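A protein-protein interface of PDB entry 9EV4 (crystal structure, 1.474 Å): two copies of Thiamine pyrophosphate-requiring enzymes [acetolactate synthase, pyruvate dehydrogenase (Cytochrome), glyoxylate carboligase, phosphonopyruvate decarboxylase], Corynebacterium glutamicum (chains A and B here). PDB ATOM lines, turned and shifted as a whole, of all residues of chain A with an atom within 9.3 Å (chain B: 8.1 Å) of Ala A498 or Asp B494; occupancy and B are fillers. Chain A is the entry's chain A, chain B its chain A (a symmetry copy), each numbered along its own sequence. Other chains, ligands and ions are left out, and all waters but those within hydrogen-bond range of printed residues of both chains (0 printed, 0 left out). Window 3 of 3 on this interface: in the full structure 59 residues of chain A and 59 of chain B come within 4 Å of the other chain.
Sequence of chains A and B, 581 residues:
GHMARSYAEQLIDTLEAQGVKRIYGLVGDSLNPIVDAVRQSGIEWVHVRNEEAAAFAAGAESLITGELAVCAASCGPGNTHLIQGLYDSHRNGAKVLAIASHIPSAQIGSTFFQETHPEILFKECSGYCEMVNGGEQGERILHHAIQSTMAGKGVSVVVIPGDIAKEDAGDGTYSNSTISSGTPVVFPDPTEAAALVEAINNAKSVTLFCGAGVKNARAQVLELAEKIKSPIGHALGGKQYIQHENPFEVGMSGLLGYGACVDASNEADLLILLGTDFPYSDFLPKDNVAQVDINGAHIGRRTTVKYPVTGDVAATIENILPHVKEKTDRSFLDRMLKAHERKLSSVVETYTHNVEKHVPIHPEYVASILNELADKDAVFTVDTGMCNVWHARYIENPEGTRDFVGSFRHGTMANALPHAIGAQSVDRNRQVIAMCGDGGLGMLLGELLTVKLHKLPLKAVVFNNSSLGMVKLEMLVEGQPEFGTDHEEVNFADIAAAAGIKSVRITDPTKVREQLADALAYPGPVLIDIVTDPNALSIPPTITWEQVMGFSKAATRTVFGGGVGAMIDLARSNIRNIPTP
Among the printed residues, merely in contact across the chains: Leu A445 with Phe B492, Leu A445 with Ile B495, Leu A449 with Val B490, Asp A494 with Ala B498, Ile A495 with Ala B498, Ala A498 with Asp B494 and Ala A498 with Ile B495.
Of the printed residues of chain B, Ala A498 touches Asn B491, Asp B494 and Ile B495. Of chain A, only Ala A498 comes within 4 Å of Asp B494. Printed residues of chain A within 4 Å of Asn B491: Ala A498 (3.5 Å). No residue of chain A comes within 4 Å of Ala B493. Ile B495 touches two residues of chain A. Of the printed residues of chain B, Ile A495 touches Ala B498 (3.5 Å). Of the printed residues of chain B, Leu A449 touches Val B490. Ala B496 touches none of the printed residues of chain A.
OD1 of Asn B491 is in hydrogen-bond range of N of Ala B493, 3.2 Å away. OD1 of Asn A491 is in hydrogen-bond range of N of Ala A493, 3.2 Å away. The backbone NH (N) of Asp A494 is in hydrogen-bond range of the side-chain amide oxygen (OD1) of Asn A491, at 2.9 Å. The guanidinium group (NH2) of Arg B505 sits at hydrogen-bond distance from the backbone carbonyl oxygen (O) of Val B490 (3.1 Å). The side-chain amide oxygen of Asn B491 is in hydrogen-bond range of the guanidinium group of Arg B505 (3.4 Å). OD1 of Asn B491 is in hydrogen-bond range of N of Asp B494 (2.9 Å).
Asn A491 touches Ala B498, and with the chains exchanged Ala A498 touches Asn B491. Asp A494 touches Ala B498, and with the chains exchanged Ala A498 touches Asp B494. Ile A495 touches Ala B498, and with the chains exchanged Ala A498 touches Ile B495. Positions printed for both chains: 448, 490, 491, 492, 493, 494, 495, 496, 497, 498, 499, 500, 501 and 503.
Of the 19 printed residues of chain B, 6 touch a printed residue of chain A. Hydrophobic or aromatic side chains of chain B that line the printed part of chain A: Val B490, Phe B492, Ile B495 and Ala B498. Of the 18 printed residues of chain A, 6 touch a printed residue of chain B. Hydrophobic or aromatic side chains of chain A within 4 Å of the printed part of chain B: Leu A445, Leu A449, Ile A495 and Ala A498.
N of Asn B491 sits at hydrogen-bond distance from O of Ala A498 (3.5 Å). The backbone NH of Asn A491 lies within hydrogen-bond range of the backbone carbonyl oxygen of Ala B498 (3.5 Å).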
ATOM      1  N   LEU A 445     -11.189   2.376   3.691  1.00  0.00           N
ATOM      2  CA  LEU A 445     -11.999   1.310   3.100  1.00  0.00           C
ATOM      3  C   LEU A 445     -11.767   1.133   1.592  1.00  0.00           C
ATOM      4  O   LEU A 445     -11.596   0.007   1.130  1.00  0.00           O
ATOM      5  CB  LEU A 445     -13.468   1.564   3.398  1.00  0.00           C
ATOM      6  CG  LEU A 445     -14.443   0.454   3.225  1.00  0.00           C
ATOM      7  CD1 LEU A 445     -13.896  -0.873   3.836  1.00  0.00           C
ATOM      8  CD2 LEU A 445     -15.810   0.837   3.890  1.00  0.00           C
ATOM      9  N   LEU A 448      -8.337  -0.457   1.039  1.00  0.00           N
ATOM     10  CA  LEU A 448      -8.321  -1.892   1.333  1.00  0.00           C
ATOM     11  C   LEU A 448      -9.041  -2.692   0.251  1.00  0.00           C
ATOM     12  O   LEU A 448      -8.617  -3.805  -0.068  1.00  0.00           O
ATOM     13  CB  LEU A 448      -8.976  -2.184   2.699  1.00  0.00           C
ATOM     14  CG  LEU A 448      -8.282  -1.586   3.922  1.00  0.00           C
ATOM     15  CD1 LEU A 448      -9.012  -1.983   5.184  1.00  0.00           C
ATOM     16  CD2 LEU A 448      -6.788  -1.986   3.977  1.00  0.00           C
ATOM     17  N   LEU A 449     -10.136  -2.147  -0.304  1.00  0.00           N
ATOM     18  CA  LEU A 449     -10.891  -2.865  -1.338  1.00  0.00           C
ATOM     19  C   LEU A 449     -10.066  -2.968  -2.647  1.00  0.00           C
ATOM     20  O   LEU A 449     -10.153  -3.984  -3.345  1.00  0.00           O
ATOM     21  CB  LEU A 449     -12.253  -2.227  -1.597  1.00  0.00           C
ATOM     22  CG  LEU A 449     -13.240  -2.312  -0.418  1.00  0.00           C
ATOM     23  CD1 LEU A 449     -14.464  -1.455  -0.693  1.00  0.00           C
ATOM     24  CD2 LEU A 449     -13.595  -3.752  -0.061  1.00  0.00           C
ATOM     25  N   LYS A 452      -7.357  -5.679  -1.873  1.00  0.00           N
ATOM     26  CA  LYS A 452      -7.989  -7.001  -1.916  1.00  0.00           C
ATOM     27  C   LYS A 452      -8.237  -7.457  -3.381  1.00  0.00           C
ATOM     28  O   LYS A 452      -7.902  -8.589  -3.736  1.00  0.00           O
ATOM     29  CB  LYS A 452      -9.324  -6.952  -1.142  1.00  0.00           C
ATOM     30  CG  LYS A 452     -10.041  -8.294  -1.083  1.00  0.00           C
ATOM     31  CD  LYS A 452     -11.535  -8.065  -0.896  1.00  0.00           C
ATOM     32  CE  LYS A 452     -12.216  -9.292  -0.351  1.00  0.00           C
ATOM     33  NZ  LYS A 452     -11.665 -10.530  -0.963  1.00  0.00           N
ATOM     34  N   VAL A 490     -11.212   2.878  17.928  1.00  0.00           N
ATOM     35  CA  VAL A 490     -11.600   2.210  16.692  1.00  0.00           C
ATOM     36  C   VAL A 490     -10.812   0.908  16.525  1.00  0.00           C
ATOM     37  O   VAL A 490      -9.613   0.894  16.780  1.00  0.00           O
ATOM     38  CB  VAL A 490     -11.354   3.155  15.483  1.00  0.00           C
ATOM     39  CG1 VAL A 490     -11.687   2.461  14.164  1.00  0.00           C
ATOM     40  CG2 VAL A 490     -12.153   4.446  15.630  1.00  0.00           C
ATOM     41  N   ASN A 491     -11.477  -0.181  16.115  1.00  0.00           N
ATOM     42  CA  ASN A 491     -10.783  -1.442  15.870  1.00  0.00           C
ATOM     43  C   ASN A 491     -10.540  -1.575  14.357  1.00  0.00           C
ATOM     44  O   ASN A 491     -11.370  -2.149  13.654  1.00  0.00           O
ATOM     45  CB  ASN A 491     -11.571  -2.645  16.448  1.00  0.00           C
ATOM     46  CG  ASN A 491     -10.763  -3.933  16.457  1.00  0.00           C
ATOM     47  OD1 ASN A 491      -9.997  -4.216  15.547  1.00  0.00           O
ATOM     48  ND2 ASN A 491     -10.924  -4.753  17.487  1.00  0.00           N
ATOM     49  N   PHE A 492      -9.399  -1.066  13.857  1.00  0.00           N
ATOM     50  CA  PHE A 492      -9.085  -1.183  12.426  1.00  0.00           C
ATOM     51  C   PHE A 492      -8.844  -2.622  11.997  1.00  0.00           C
ATOM     52  O   PHE A 492      -9.114  -2.949  10.840  1.00  0.00           O
ATOM     53  CB  PHE A 492      -7.888  -0.304  12.028  1.00  0.00           C
ATOM     54  CG  PHE A 492      -8.209   1.157  12.180  1.00  0.00           C
ATOM     55  CD1 PHE A 492      -8.892   1.843  11.184  1.00  0.00           C
ATOM     56  CD2 PHE A 492      -7.834   1.851  13.316  1.00  0.00           C
ATOM     57  CE1 PHE A 492      -9.179   3.192  11.320  1.00  0.00           C
ATOM     58  CE2 PHE A 492      -8.115   3.200  13.443  1.00  0.00           C
ATOM     59  CZ  PHE A 492      -8.787   3.863  12.444  1.00  0.00           C
ATOM     60  N   ALA A 493      -8.377  -3.505  12.912  1.00  0.00           N
ATOM     61  CA  ALA A 493      -8.213  -4.913  12.546  1.00  0.00           C
ATOM     62  C   ALA A 493      -9.577  -5.543  12.169  1.00  0.00           C
ATOM     63  O   ALA A 493      -9.655  -6.276  11.172  1.00  0.00           O
ATOM     64  CB  ALA A 493      -7.553  -5.701  13.682  1.00  0.00           C
ATOM     65  N   ASP A 494     -10.657  -5.190  12.901  1.00  0.00           N
ATOM     66  CA  ASP A 494     -12.007  -5.710  12.628  1.00  0.00           C
ATOM     67  C   ASP A 494     -12.553  -5.143  11.321  1.00  0.00           C
ATOM     68  O   ASP A 494     -13.224  -5.851  10.569  1.00  0.00           O
ATOM     69  CB  ASP A 494     -12.975  -5.416  13.792  1.00  0.00           C
ATOM     70  CG  ASP A 494     -12.791  -6.344  14.996  1.00  0.00           C
ATOM     71  OD1 ASP A 494     -11.970  -7.305  14.904  1.00  0.00           O
ATOM     72  OD2 ASP A 494     -13.462  -6.121  16.022  1.00  0.00           O
ATOM     73  N   ILE A 495     -12.270  -3.861  11.042  1.00  0.00           N
ATOM     74  CA  ILE A 495     -12.697  -3.229   9.798  1.00  0.00           C
ATOM     75  C   ILE A 495     -12.024  -3.932   8.627  1.00  0.00           C
ATOM     76  O   ILE A 495     -12.703  -4.310   7.673  1.00  0.00           O
ATOM     77  CB  ILE A 495     -12.351  -1.719   9.843  1.00  0.00           C
ATOM     78  CG1 ILE A 495     -13.221  -1.019  10.880  1.00  0.00           C
ATOM     79  CG2 ILE A 495     -12.469  -1.079   8.466  1.00  0.00           C
ATOM     80  CD1 ILE A 495     -12.779   0.427  11.218  1.00  0.00           C
ATOM     81  N   ALA A 496     -10.693  -4.163   8.722  1.00  0.00           N
ATOM     82  CA  ALA A 496      -9.973  -4.849   7.654  1.00  0.00           C
ATOM     83  C   ALA A 496     -10.519  -6.277   7.450  1.00  0.00           C
ATOM     84  O   ALA A 496     -10.803  -6.660   6.312  1.00  0.00           O
ATOM     85  CB  ALA A 496      -8.480  -4.894   7.954  1.00  0.00           C
ATOM     86  N   ALA A 497     -10.752  -7.017   8.545  1.00  0.00           N
ATOM     87  CA  ALA A 497     -11.310  -8.373   8.466  1.00  0.00           C
ATOM     88  C   ALA A 497     -12.702  -8.377   7.800  1.00  0.00           C
ATOM     89  O   ALA A 497     -12.987  -9.270   7.012  1.00  0.00           O
ATOM     90  CB  ALA A 497     -11.396  -8.991   9.857  1.00  0.00           C
ATOM     91  N   ALA A 498     -13.547  -7.354   8.066  1.00  0.00           N
ATOM     92  CA  ALA A 498     -14.878  -7.259   7.434  1.00  0.00           C
ATOM     93  C   ALA A 498     -14.781  -6.965   5.946  1.00  0.00           C
ATOM     94  O   ALA A 498     -15.679  -7.329   5.185  1.00  0.00           O
ATOM     95  CB  ALA A 498     -15.711  -6.181   8.112  1.00  0.00           C
ATOM     96  N   ALA A 499     -13.727  -6.256   5.525  1.00  0.00           N
ATOM     97  CA  ALA A 499     -13.520  -5.966   4.110  1.00  0.00           C
ATOM     98  C   ALA A 499     -12.776  -7.122   3.377  1.00  0.00           C
ATOM     99  O   ALA A 499     -12.468  -6.975   2.205  1.00  0.00           O
ATOM    100  CB  ALA A 499     -12.749  -4.655   3.944  1.00  0.00           C
ATOM    101  N   GLY A 500     -12.500  -8.242   4.052  1.00  0.00           N
ATOM    102  CA  GLY A 500     -11.833  -9.389   3.455  1.00  0.00           C
ATOM    103  C   GLY A 500     -10.312  -9.325   3.434  1.00  0.00           C
ATOM    104  O   GLY A 500      -9.681  -9.983   2.606  1.00  0.00           O
ATOM    105  N   ILE A 501      -9.707  -8.572   4.362  1.00  0.00           N
ATOM    106  CA  ILE A 501      -8.256  -8.453   4.460  1.00  0.00           C
ATOM    107  C   ILE A 501      -7.769  -9.087   5.777  1.00  0.00           C
ATOM    108  O   ILE A 501      -8.349  -8.803   6.827  1.00  0.00           O
ATOM    109  CB  ILE A 501      -7.869  -6.935   4.412  1.00  0.00           C
ATOM    110  CG1 ILE A 501      -8.310  -6.255   3.077  1.00  0.00           C
ATOM    111  CG2 ILE A 501      -6.376  -6.700   4.721  1.00  0.00           C
ATOM    112  CD1 ILE A 501      -7.520  -6.698   1.897  1.00  0.00           C
ATOM    113  N   LYS A 502      -6.683  -9.874   5.743  1.00  0.00           N
ATOM    114  CA  LYS A 502      -6.040 -10.441   6.937  1.00  0.00           C
ATOM    115  C   LYS A 502      -5.627  -9.287   7.866  1.00  0.00           C
ATOM    116  O   LYS A 502      -5.099  -8.282   7.388  1.00  0.00           O
ATOM    117  CB  LYS A 502      -4.809 -11.273   6.528  1.00  0.00           C
ATOM    118  CG  LYS A 502      -3.946 -11.828   7.648  1.00  0.00           C
ATOM    119  CD  LYS A 502      -4.687 -12.896   8.460  1.00  0.00           C
ATOM    120  CE  LYS A 502      -3.779 -13.624   9.426  1.00  0.00           C
ATOM    121  NZ  LYS A 502      -2.750 -12.714   9.978  1.00  0.00           N
ATOM    122  N   SER A 503      -5.865  -9.428   9.168  1.00  0.00           N
ATOM    123  CA  SER A 503      -5.494  -8.378  10.095  1.00  0.00           C
ATOM    124  C   SER A 503      -5.000  -8.942  11.439  1.00  0.00           C
ATOM    125  O   SER A 503      -5.281 -10.088  11.807  1.00  0.00           O
ATOM    126  CB  SER A 503      -6.676  -7.429  10.312  1.00  0.00           C
ATOM    127  OG  SER A 503      -7.681  -8.089  11.066  1.00  0.00           O
ATOM    128  N   LEU B 448     -18.457   7.817   8.921  1.00  0.00           N
ATOM    129  CA  LEU B 448     -19.000   7.181  10.124  1.00  0.00           C
ATOM    130  C   LEU B 448     -18.344   7.728  11.390  1.00  0.00           C
ATOM    131  O   LEU B 448     -19.017   7.865  12.414  1.00  0.00           O
ATOM    132  CB  LEU B 448     -18.808   5.651  10.075  1.00  0.00           C
ATOM    133  CG  LEU B 448     -19.538   4.914   8.953  1.00  0.00           C
ATOM    134  CD1 LEU B 448     -19.287   3.428   9.052  1.00  0.00           C
ATOM    135  CD2 LEU B 448     -21.050   5.240   8.952  1.00  0.00           C
ATOM    136  N   GLU B 489     -17.717 -10.292  -1.303  1.00  0.00           N
ATOM    137  CA  GLU B 489     -18.811  -9.641  -0.589  1.00  0.00           C
ATOM    138  C   GLU B 489     -18.282  -8.889   0.637  1.00  0.00           C
ATOM    139  O   GLU B 489     -17.519  -9.457   1.423  1.00  0.00           O
ATOM    140  CB  GLU B 489     -19.872 -10.671  -0.174  1.00  0.00           C
ATOM    141  N   VAL B 490     -18.662  -7.622   0.783  1.00  0.00           N
ATOM    142  CA  VAL B 490     -18.232  -6.794   1.903  1.00  0.00           C
ATOM    143  C   VAL B 490     -19.335  -6.728   2.964  1.00  0.00           C
ATOM    144  O   VAL B 490     -20.500  -6.579   2.611  1.00  0.00           O
ATOM    145  CB  VAL B 490     -17.876  -5.368   1.399  1.00  0.00           C
ATOM    146  CG1 VAL B 490     -17.486  -4.454   2.558  1.00  0.00           C
ATOM    147  CG2 VAL B 490     -16.762  -5.423   0.357  1.00  0.00           C
ATOM    148  N   ASN B 491     -18.978  -6.850   4.250  1.00  0.00           N
ATOM    149  CA  ASN B 491     -19.963  -6.733   5.321  1.00  0.00           C
ATOM    150  C   ASN B 491     -19.878  -5.311   5.902  1.00  0.00           C
ATOM    151  O   ASN B 491     -19.137  -5.086   6.858  1.00  0.00           O
ATOM    152  CB  ASN B 491     -19.760  -7.825   6.402  1.00  0.00           C
ATOM    153  CG  ASN B 491     -20.916  -7.908   7.386  1.00  0.00           C
ATOM    154  OD1 ASN B 491     -21.500  -6.907   7.776  1.00  0.00           O
ATOM    155  ND2 ASN B 491     -21.270  -9.111   7.817  1.00  0.00           N
ATOM    156  N   PHE B 492     -20.647  -4.358   5.345  1.00  0.00           N
ATOM    157  CA  PHE B 492     -20.641  -2.983   5.868  1.00  0.00           C
ATOM    158  C   PHE B 492     -21.225  -2.890   7.269  1.00  0.00           C
ATOM    159  O   PHE B 492     -20.814  -2.008   8.024  1.00  0.00           O
ATOM    160  CB  PHE B 492     -21.367  -2.009   4.926  1.00  0.00           C
ATOM    161  CG  PHE B 492     -20.639  -1.870   3.617  1.00  0.00           C
ATOM    162  CD1 PHE B 492     -19.561  -1.004   3.491  1.00  0.00           C
ATOM    163  CD2 PHE B 492     -21.024  -2.605   2.510  1.00  0.00           C
ATOM    164  CE1 PHE B 492     -18.896  -0.870   2.282  1.00  0.00           C
ATOM    165  CE2 PHE B 492     -20.363  -2.460   1.303  1.00  0.00           C
ATOM    166  CZ  PHE B 492     -19.302  -1.593   1.197  1.00  0.00           C
ATOM    167  N   ALA B 493     -22.149  -3.802   7.653  1.00  0.00           N
ATOM    168  CA  ALA B 493     -22.666  -3.783   9.022  1.00  0.00           C
ATOM    169  C   ALA B 493     -21.528  -4.041  10.041  1.00  0.00           C
ATOM    170  O   ALA B 493     -21.460  -3.348  11.067  1.00  0.00           O
ATOM    171  CB  ALA B 493     -23.789  -4.811   9.199  1.00  0.00           C
ATOM    172  N   ASP B 494     -20.593  -4.962   9.720  1.00  0.00           N
ATOM    173  CA  ASP B 494     -19.457  -5.281  10.600  1.00  0.00           C
ATOM    174  C   ASP B 494     -18.470  -4.118  10.657  1.00  0.00           C
ATOM    175  O   ASP B 494     -17.906  -3.832  11.714  1.00  0.00           O
ATOM    176  CB  ASP B 494     -18.743  -6.575  10.159  1.00  0.00           C
ATOM    177  CG  ASP B 494     -19.488  -7.854  10.551  1.00  0.00           C
ATOM    178  OD1 ASP B 494     -20.529  -7.757  11.267  1.00  0.00           O
ATOM    179  OD2 ASP B 494     -19.038  -8.946  10.152  1.00  0.00           O
ATOM    180  N   ILE B 495     -18.254  -3.440   9.517  1.00  0.00           N
ATOM    181  CA  ILE B 495     -17.371  -2.280   9.466  1.00  0.00           C
ATOM    182  C   ILE B 495     -17.944  -1.180  10.350  1.00  0.00           C
ATOM    183  O   ILE B 495     -17.219  -0.627  11.178  1.00  0.00           O
ATOM    184  CB  ILE B 495     -17.215  -1.817   7.995  1.00  0.00           C
ATOM    185  CG1 ILE B 495     -16.432  -2.859   7.204  1.00  0.00           C
ATOM    186  CG2 ILE B 495     -16.582  -0.435   7.910  1.00  0.00           C
ATOM    187  CD1 ILE B 495     -16.453  -2.650   5.670  1.00  0.00           C
ATOM    188  N   ALA B 496     -19.262  -0.900  10.220  1.00  0.00           N
ATOM    189  CA  ALA B 496     -19.895   0.126  11.042  1.00  0.00           C
ATOM    190  C   ALA B 496     -19.804  -0.235  12.539  1.00  0.00           C
ATOM    191  O   ALA B 496     -19.402   0.611  13.342  1.00  0.00           O
ATOM    192  CB  ALA B 496     -21.351   0.319  10.635  1.00  0.00           C
ATOM    193  N   ALA B 497     -20.081  -1.499  12.893  1.00  0.00           N
ATOM    194  CA  ALA B 497     -19.985  -1.958  14.285  1.00  0.00           C
ATOM    195  C   ALA B 497     -18.553  -1.799  14.838  1.00  0.00           C
ATOM    196  O   ALA B 497     -18.395  -1.405  15.987  1.00  0.00           O
ATOM    197  CB  ALA B 497     -20.427  -3.414  14.393  1.00  0.00           C
ATOM    198  N   ALA B 498     -17.511  -2.047  14.012  1.00  0.00           N
ATOM    199  CA  ALA B 498     -16.112  -1.873  14.449  1.00  0.00           C
ATOM    200  C   ALA B 498     -15.762  -0.410  14.667  1.00  0.00           C
ATOM    201  O   ALA B 498     -14.877  -0.099  15.467  1.00  0.00           O
ATOM    202  CB  ALA B 498     -15.159  -2.477  13.429  1.00  0.00           C
ATOM    203  N   ALA B 499     -16.405   0.495  13.921  1.00  0.00           N
ATOM    204  CA  ALA B 499     -16.175   1.926  14.092  1.00  0.00           C
ATOM    205  C   ALA B 499     -17.058   2.532  15.223  1.00  0.00           C
ATOM    206  O   ALA B 499     -17.022   3.736  15.418  1.00  0.00           O
ATOM    207  CB  ALA B 499     -16.424   2.665  12.775  1.00  0.00           C
ATOM    208  N   GLY B 500     -17.827   1.714  15.949  1.00  0.00           N
ATOM    209  CA  GLY B 500     -18.670   2.174  17.043  1.00  0.00           C
ATOM    210  C   GLY B 500     -20.041   2.697  16.639  1.00  0.00           C
ATOM    211  O   GLY B 500     -20.639   3.483  17.375  1.00  0.00           O
ATOM    212  N   ILE B 501     -20.570   2.242  15.496  1.00  0.00           N
ATOM    213  CA  ILE B 501     -21.887   2.648  15.017  1.00  0.00           C
ATOM    214  C   ILE B 501     -22.843   1.440  15.033  1.00  0.00           C
ATOM    215  O   ILE B 501     -22.462   0.372  14.550  1.00  0.00           O
ATOM    216  CB  ILE B 501     -21.745   3.211  13.562  1.00  0.00           C
ATOM    217  CG1 ILE B 501     -20.812   4.462  13.501  1.00  0.00           C
ATOM    218  CG2 ILE B 501     -23.112   3.469  12.896  1.00  0.00           C
ATOM    219  CD1 ILE B 501     -21.406   5.675  14.124  1.00  0.00           C
ATOM    220  N   SER B 503     -25.487  -1.127  13.744  1.00  0.00           N
ATOM    221  CA  SER B 503     -25.706  -1.579  12.385  1.00  0.00           C
ATOM    222  C   SER B 503     -26.652  -2.791  12.325  1.00  0.00           C
ATOM    223  O   SER B 503     -26.847  -3.515  13.309  1.00  0.00           O
ATOM    224  CB  SER B 503     -24.366  -1.909  11.721  1.00  0.00           C
ATOM    225  OG  SER B 503     -23.830  -3.090  12.297  1.00  0.00           O
ATOM    226  N   VAL B 504     -27.228  -3.005  11.139  1.00  0.00           N
ATOM    227  CA  VAL B 504     -28.081  -4.152  10.870  1.00  0.00           C
ATOM    228  C   VAL B 504     -27.793  -4.665   9.453  1.00  0.00           C
ATOM    229  O   VAL B 504     -27.442  -3.867   8.559  1.00  0.00           O
ATOM    230  CB  VAL B 504     -29.587  -3.855  11.078  1.00  0.00           C
ATOM    231  CG1 VAL B 504     -30.104  -2.846  10.083  1.00  0.00           C
ATOM    232  CG2 VAL B 504     -30.394  -5.142  10.997  1.00  0.00           C
ATOM    233  N   ARG B 505     -27.879  -5.997   9.255  1.00  0.00           N
ATOM    234  CA  ARG B 505     -27.659  -6.548   7.925  1.00  0.00           C
ATOM    235  C   ARG B 505     -28.957  -7.193   7.431  1.00  0.00           C
ATOM    236  O   ARG B 505     -29.526  -8.031   8.128  1.00  0.00           O
ATOM    237  CB  ARG B 505     -26.477  -7.539   7.918  1.00  0.00           C
ATOM    238  CG  ARG B 505     -25.815  -7.632   6.540  1.00  0.00           C
ATOM    239  CD  ARG B 505     -24.417  -8.180   6.626  1.00  0.00           C
ATOM    240  NE  ARG B 505     -23.644  -7.924   5.406  1.00  0.00           N
ATOM    241  CZ  ARG B 505     -23.513  -8.792   4.408  1.00  0.00           C
ATOM    242  NH1 ARG B 505     -24.114  -9.976   4.465  1.00  0.00           N
ATOM    243  NH2 ARG B 505     -22.789  -8.481   3.340  1.00  0.00           N
ATOM    244  N   LEU B 527     -26.204   2.174  10.467  1.00  0.00           N
ATOM    245  CA  LEU B 527     -25.858   1.819   9.102  1.00  0.00           C
ATOM    246  C   LEU B 527     -26.644   0.539   8.794  1.00  0.00           C
ATOM    247  O   LEU B 527     -26.593  -0.441   9.567  1.00  0.00           O
ATOM    248  CB  LEU B 527     -24.352   1.660   8.849  1.00  0.00           C
ATOM    249  CG  LEU B 527     -23.996   1.242   7.399  1.00  0.00           C
ATOM    250  CD1 LEU B 527     -22.619   1.797   6.968  1.00  0.00           C
ATOM    251  CD2 LEU B 527     -23.970  -0.322   7.235  1.00  0.00           C
ATOM    252  N   ASP B 529     -27.095  -2.279   6.204  1.00  0.00           N
ATOM    253  CA  ASP B 529     -26.409  -2.949   5.111  1.00  0.00           C
ATOM    254  C   ASP B 529     -27.373  -3.908   4.429  1.00  0.00           C
ATOM    255  O   ASP B 529     -27.637  -4.977   4.977  1.00  0.00           O
ATOM    256  CB  ASP B 529     -25.205  -3.682   5.698  1.00  0.00           C
ATOM    257  CG  ASP B 529     -24.357  -4.457   4.714  1.00  0.00           C
ATOM    258  OD1 ASP B 529     -24.631  -4.364   3.490  1.00  0.00           O
ATOM    259  OD2 ASP B 529     -23.407  -5.156   5.171  1.00  0.00           O
